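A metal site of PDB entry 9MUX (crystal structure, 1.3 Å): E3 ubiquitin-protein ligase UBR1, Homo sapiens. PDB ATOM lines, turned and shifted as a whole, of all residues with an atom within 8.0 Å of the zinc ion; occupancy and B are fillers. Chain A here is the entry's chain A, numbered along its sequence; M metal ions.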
ATOM      1  N   SER A  20      11.993  11.074  16.290  1.00  0.00           N
ATOM      2  CA  SER A  20      13.050  10.290  15.669  1.00  0.00           C
ATOM      3  C   SER A  20      12.396   9.384  14.642  1.00  0.00           C
ATOM      4  O   SER A  20      11.312   8.847  14.880  1.00  0.00           O
ATOM      5  CB  SER A  20      13.817   9.465  16.694  1.00  0.00           C
ATOM      6  OG  SER A  20      14.909   8.820  16.049  1.00  0.00           O
ATOM      7  N   CYS A  21      13.023   9.239  13.496  1.00  0.00           N
ATOM      8  CA  CYS A  21      12.563   8.278  12.517  1.00  0.00           C
ATOM      9  C   CYS A  21      13.185   6.933  12.864  1.00  0.00           C
ATOM     10  O   CYS A  21      14.413   6.782  12.800  1.00  0.00           O
ATOM     11  CB  CYS A  21      12.980   8.659  11.102  1.00  0.00           C
ATOM     12  SG  CYS A  21      12.284   7.452   9.992  1.00  0.00           S
ATOM     13  N   ARG A  22      12.353   5.973  13.223  1.00  0.00           N
ATOM     14  CA  ARG A  22      12.879   4.669  13.561  1.00  0.00           C
ATOM     15  C   ARG A  22      13.400   3.922  12.341  1.00  0.00           C
ATOM     16  O   ARG A  22      14.283   3.071  12.480  1.00  0.00           O
ATOM     17  CB  ARG A  22      11.820   3.854  14.286  1.00  0.00           C
ATOM     18  CG  ARG A  22      11.328   4.635  15.481  1.00  0.00           C
ATOM     19  CD  ARG A  22      10.382   3.862  16.325  1.00  0.00           C
ATOM     20  NE  ARG A  22      10.995   2.623  16.772  1.00  0.00           N
ATOM     21  CZ  ARG A  22      10.375   1.756  17.538  1.00  0.00           C
ATOM     22  NH1 ARG A  22       9.130   1.950  17.932  1.00  0.00           N
ATOM     23  NH2 ARG A  22      11.010   0.645  17.904  1.00  0.00           N
ATOM     24  N   ASP A  23      12.896   4.245  11.156  1.00  0.00           N
ATOM     25  CA  ASP A  23      13.399   3.609   9.942  1.00  0.00           C
ATOM     26  C   ASP A  23      14.749   4.157   9.518  1.00  0.00           C
ATOM     27  O   ASP A  23      15.550   3.417   8.941  1.00  0.00           O
ATOM     28  CB  ASP A  23      12.398   3.787   8.796  1.00  0.00           C
ATOM     29  CG  ASP A  23      11.068   3.117   9.059  1.00  0.00           C
ATOM     30  OD1 ASP A  23      11.071   2.052   9.714  1.00  0.00           O
ATOM     31  OD2 ASP A  23      10.042   3.669   8.634  1.00  0.00           O
ATOM     32  N   CYS A  24      15.023   5.440   9.763  1.00  0.00           N
ATOM     33  CA  CYS A  24      16.213   6.056   9.182  1.00  0.00           C
ATOM     34  C   CYS A  24      17.263   6.480  10.200  1.00  0.00           C
ATOM     35  O   CYS A  24      18.387   6.733   9.793  1.00  0.00           O
ATOM     36  CB  CYS A  24      15.828   7.281   8.352  1.00  0.00           C
ATOM     37  SG  CYS A  24      14.661   6.932   7.021  1.00  0.00           S
ATOM     38  N   ALA A  25      16.922   6.572  11.476  1.00  0.00           N
ATOM     39  CA  ALA A  25      17.902   7.018  12.467  1.00  0.00           C
ATOM     40  C   ALA A  25      19.060   6.032  12.533  1.00  0.00           C
ATOM     41  O   ALA A  25      18.850   4.818  12.601  1.00  0.00           O
ATOM     42  CB  ALA A  25      17.246   7.095  13.836  1.00  0.00           C
ATOM     43  N   LEU A  32      14.809  14.957  15.455  1.00  0.00           N
ATOM     44  CA  LEU A  32      14.417  16.117  14.683  1.00  0.00           C
ATOM     45  C   LEU A  32      13.437  16.945  15.500  1.00  0.00           C
ATOM     46  O   LEU A  32      12.630  16.398  16.262  1.00  0.00           O
ATOM     47  CB  LEU A  32      13.710  15.682  13.413  1.00  0.00           C
ATOM     48  CG  LEU A  32      14.568  14.948  12.352  1.00  0.00           C
ATOM     49  CD1 LEU A  32      13.667  14.408  11.233  1.00  0.00           C
ATOM     50  CD2 LEU A  32      15.656  15.831  11.775  1.00  0.00           C
ATOM     51  N   PHE A  37      10.851  17.561  11.166  1.00  0.00           N
ATOM     52  CA  PHE A  37      10.178  16.278  10.959  1.00  0.00           C
ATOM     53  C   PHE A  37       9.044  16.435   9.947  1.00  0.00           C
ATOM     54  O   PHE A  37       8.946  15.670   8.982  1.00  0.00           O
ATOM     55  CB  PHE A  37       9.638  15.766  12.294  1.00  0.00           C
ATOM     56  CG  PHE A  37       8.860  14.502  12.167  1.00  0.00           C
ATOM     57  CD1 PHE A  37       9.502  13.299  11.932  1.00  0.00           C
ATOM     58  CD2 PHE A  37       7.483  14.506  12.296  1.00  0.00           C
ATOM     59  CE1 PHE A  37       8.779  12.112  11.824  1.00  0.00           C
ATOM     60  CE2 PHE A  37       6.774  13.322  12.189  1.00  0.00           C
ATOM     61  CZ  PHE A  37       7.425  12.141  11.951  1.00  0.00           C
ATOM     62  N   SER A  40      10.000  16.877   6.328  1.00  0.00           N
ATOM     63  CA  SER A  40      10.928  15.858   5.856  1.00  0.00           C
ATOM     64  C   SER A  40      10.151  14.622   5.404  1.00  0.00           C
ATOM     65  O   SER A  40       8.983  14.431   5.729  1.00  0.00           O
ATOM     66  CB  SER A  40      11.916  15.443   6.954  1.00  0.00           C
ATOM     67  OG  SER A  40      11.302  14.546   7.868  1.00  0.00           O
ATOM     68  N   VAL A  41      10.879  13.719   4.739  1.00  0.00           N
ATOM     69  CA  VAL A  41      10.293  12.473   4.294  1.00  0.00           C
ATOM     70  C   VAL A  41       9.875  11.604   5.467  1.00  0.00           C
ATOM     71  O   VAL A  41       9.003  10.732   5.334  1.00  0.00           O
ATOM     72  CB  VAL A  41      11.285  11.718   3.382  1.00  0.00           C
ATOM     73  CG1 VAL A  41      12.486  11.197   4.201  1.00  0.00           C
ATOM     74  CG2 VAL A  41      10.590  10.574   2.649  1.00  0.00           C
ATOM     75  N   HIS A  42      10.462  11.824   6.640  1.00  0.00           N
ATOM     76  CA  HIS A  42      10.282  10.928   7.766  1.00  0.00           C
ATOM     77  C   HIS A  42       8.905  11.061   8.378  1.00  0.00           C
ATOM     78  O   HIS A  42       8.501  10.166   9.119  1.00  0.00           O
ATOM     79  CB  HIS A  42      11.376  11.149   8.812  1.00  0.00           C
ATOM     80  CG  HIS A  42      12.736  11.157   8.195  1.00  0.00           C
ATOM     81  ND1 HIS A  42      13.328  10.019   7.700  1.00  0.00           N
ATOM     82  CD2 HIS A  42      13.569  12.179   7.914  1.00  0.00           C
ATOM     83  CE1 HIS A  42      14.490  10.335   7.165  1.00  0.00           C
ATOM     84  NE2 HIS A  42      14.665  11.641   7.283  1.00  0.00           N
ATOM     85  N   LYS A  43       8.152  12.116   8.016  1.00  0.00           N
ATOM     86  CA  LYS A  43       6.763  12.208   8.425  1.00  0.00           C
ATOM     87  C   LYS A  43       5.954  11.017   7.902  1.00  0.00           C
ATOM     88  O   LYS A  43       4.880  10.729   8.428  1.00  0.00           O
ATOM     89  CB  LYS A  43       6.174  13.503   7.894  1.00  0.00           C
ATOM     90  CG  LYS A  43       5.953  13.492   6.383  1.00  0.00           C
ATOM     91  CD  LYS A  43       5.449  14.829   5.870  1.00  0.00           C
ATOM     92  CE  LYS A  43       5.083  14.720   4.403  1.00  0.00           C
ATOM     93  NZ  LYS A  43       4.419  15.963   3.919  1.00  0.00           N
ATOM     94  N   ASN A  44       6.464  10.317   6.890  1.00  0.00           N
ATOM     95  CA  ASN A  44       5.789   9.176   6.292  1.00  0.00           C
ATOM     96  C   ASN A  44       6.357   7.848   6.771  1.00  0.00           C
ATOM     97  O   ASN A  44       5.989   6.794   6.235  1.00  0.00           O
ATOM     98  CB  ASN A  44       5.867   9.259   4.764  1.00  0.00           C
ATOM     99  CG  ASN A  44       4.979  10.368   4.183  1.00  0.00           C
ATOM    100  OD1 ASN A  44       4.132  10.919   4.884  1.00  0.00           O
ATOM    101  ND2 ASN A  44       5.179  10.680   2.914  1.00  0.00           N
ATOM    102  N   HIS A  45       7.265   7.862   7.738  1.00  0.00           N
ATOM    103  CA  HIS A  45       7.963   6.663   8.189  1.00  0.00           C
ATOM    104  C   HIS A  45       7.512   6.272   9.583  1.00  0.00           C
ATOM    105  O   HIS A  45       6.754   6.982  10.244  1.00  0.00           O
ATOM    106  CB  HIS A  45       9.473   6.942   8.176  1.00  0.00           C
ATOM    107  CG  HIS A  45      10.017   7.109   6.801  1.00  0.00           C
ATOM    108  ND1 HIS A  45      11.297   7.542   6.554  1.00  0.00           N
ATOM    109  CD2 HIS A  45       9.465   6.860   5.589  1.00  0.00           C
ATOM    110  CE1 HIS A  45      11.502   7.572   5.250  1.00  0.00           C
ATOM    111  NE2 HIS A  45      10.406   7.163   4.643  1.00  0.00           N
ATOM    112  N   ARG A  46       8.002   5.133  10.055  1.00  0.00           N
ATOM    113  CA  ARG A  46       7.785   4.762  11.447  1.00  0.00           C
ATOM    114  C   ARG A  46       8.591   5.701  12.317  1.00  0.00           C
ATOM    115  O   ARG A  46       9.799   5.838  12.129  1.00  0.00           O
ATOM    116  CB  ARG A  46       8.268   3.325  11.644  1.00  0.00           C
ATOM    117  CG  ARG A  46       8.020   2.737  13.013  1.00  0.00           C
ATOM    118  CD  ARG A  46       8.719   1.406  13.110  1.00  0.00           C
ATOM    119  NE  ARG A  46       8.464   0.718  14.364  1.00  0.00           N
ATOM    120  CZ  ARG A  46       9.256  -0.216  14.861  1.00  0.00           C
ATOM    121  NH1 ARG A  46      10.413  -0.504  14.299  1.00  0.00           N
ATOM    122  NH2 ARG A  46       8.864  -0.875  15.950  1.00  0.00           N
ATOM    123  N   TYR A  47       7.942   6.343  13.283  1.00  0.00           N
ATOM    124  CA  TYR A  47       8.597   7.373  14.080  1.00  0.00           C
ATOM    125  C   TYR A  47       8.259   7.224  15.552  1.00  0.00           C
ATOM    126  O   TYR A  47       7.297   6.559  15.932  1.00  0.00           O
ATOM    127  CB  TYR A  47       8.233   8.796  13.588  1.00  0.00           C
ATOM    128  CG  TYR A  47       6.795   9.178  13.787  1.00  0.00           C
ATOM    129  CD1 TYR A  47       5.819   8.747  12.901  1.00  0.00           C
ATOM    130  CD2 TYR A  47       6.408   9.976  14.861  1.00  0.00           C
ATOM    131  CE1 TYR A  47       4.505   9.090  13.065  1.00  0.00           C
ATOM    132  CE2 TYR A  47       5.078  10.327  15.038  1.00  0.00           C
ATOM    133  CZ  TYR A  47       4.123   9.867  14.129  1.00  0.00           C
ATOM    134  OH  TYR A  47       2.798  10.193  14.267  1.00  0.00           O
ATOM    135  N   TRP A  66      21.215  10.037   9.606  1.00  0.00           N
ATOM    136  CA  TRP A  66      20.038   9.562   8.870  1.00  0.00           C
ATOM    137  C   TRP A  66      20.490   8.703   7.698  1.00  0.00           C
ATOM    138  O   TRP A  66      21.315   9.134   6.888  1.00  0.00           O
ATOM    139  CB  TRP A  66      19.193  10.741   8.353  1.00  0.00           C
ATOM    140  CG  TRP A  66      18.864  11.700   9.458  1.00  0.00           C
ATOM    141  CD1 TRP A  66      19.385  12.947   9.651  1.00  0.00           C
ATOM    142  CD2 TRP A  66      17.984  11.452  10.556  1.00  0.00           C
ATOM    143  NE1 TRP A  66      18.865  13.498  10.797  1.00  0.00           N
ATOM    144  CE2 TRP A  66      18.013  12.596  11.383  1.00  0.00           C
ATOM    145  CE3 TRP A  66      17.187  10.367  10.925  1.00  0.00           C
ATOM    146  CZ2 TRP A  66      17.281  12.690  12.547  1.00  0.00           C
ATOM    147  CZ3 TRP A  66      16.458  10.451  12.091  1.00  0.00           C
ATOM    148  CH2 TRP A  66      16.506  11.607  12.895  1.00  0.00           C
ATOM    149  N   LYS A  67      19.873   7.527   7.571  1.00  0.00           N
ATOM    150  CA  LYS A  67      20.207   6.640   6.464  1.00  0.00           C
ATOM    151  C   LYS A  67      19.738   7.200   5.134  1.00  0.00           C
ATOM    152  O   LYS A  67      20.385   6.961   4.101  1.00  0.00           O
ATOM    153  CB  LYS A  67      19.590   5.267   6.706  1.00  0.00           C
ATOM    154  CG  LYS A  67      20.225   4.547   7.876  1.00  0.00           C
ATOM    155  CD  LYS A  67      19.890   3.080   7.896  1.00  0.00           C
ATOM    156  CE  LYS A  67      18.681   2.810   8.759  1.00  0.00           C
ATOM    157  NZ  LYS A  67      19.033   2.819  10.202  1.00  0.00           N
ATOM    158  N   THR A  68      18.645   7.950   5.130  1.00  0.00           N
ATOM    159  CA  THR A  68      18.113   8.596   3.930  1.00  0.00           C
ATOM    160  C   THR A  68      17.491   9.907   4.380  1.00  0.00           C
ATOM    161  O   THR A  68      17.100  10.064   5.539  1.00  0.00           O
ATOM    162  CB  THR A  68      17.019   7.750   3.217  1.00  0.00           C
ATOM    163  OG1 THR A  68      15.742   7.958   3.836  1.00  0.00           O
ATOM    164  CG2 THR A  68      17.333   6.262   3.238  1.00  0.00           C
ATOM    165  N   GLY A  69      17.374  10.835   3.440  1.00  0.00           N
ATOM    166  CA  GLY A  69      16.678  12.086   3.653  1.00  0.00           C
ATOM    167  C   GLY A  69      17.136  12.892   4.859  1.00  0.00           C
ATOM    168  O   GLY A  69      16.344  13.262   5.728  1.00  0.00           O
HETATM  169 ZN    ZN M   1      12.801   8.008   7.822  1.00  0.00          ZN
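The backbone carbonyl oxygen (O) of Gly 69 sits at hydrogen-bond distance from a ring nitrogen (NE2) of His 42, 2.8 Å away. The side-chain sulfur (SG) of Cys 21 lies close to the backbone NH (N) of Asp 23 (3.5 Å). The backbone carbonyl oxygen of Cys 24 sits at hydrogen-bond distance from the backbone NH of Lys 67, 2.8 Å away. N of His 42 sits close to OG of Ser 40, at 3.1 Å. The backbone carbonyl oxygen (O) of Arg 46 sits close to the side-chain sulfur (SG) of Cys 21. The side-chain sulfur of Cys 24 lies close to the side-chain hydroxyl of Thr 68 (3.5 Å). The backbone carbonyl oxygen (O) of Thr 68 sits close to a ring nitrogen (NE2) of His 42, at 3.4 Å.
The zinc ion is bound by ND1 of His 45 (2.0 Å), ND1 of His 42 (2.1 Å), SG of Cys 24 (2.3 Å) and SG of Cys 21 (2.3 Å). The zinc ion has four donor atoms within binding distance.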
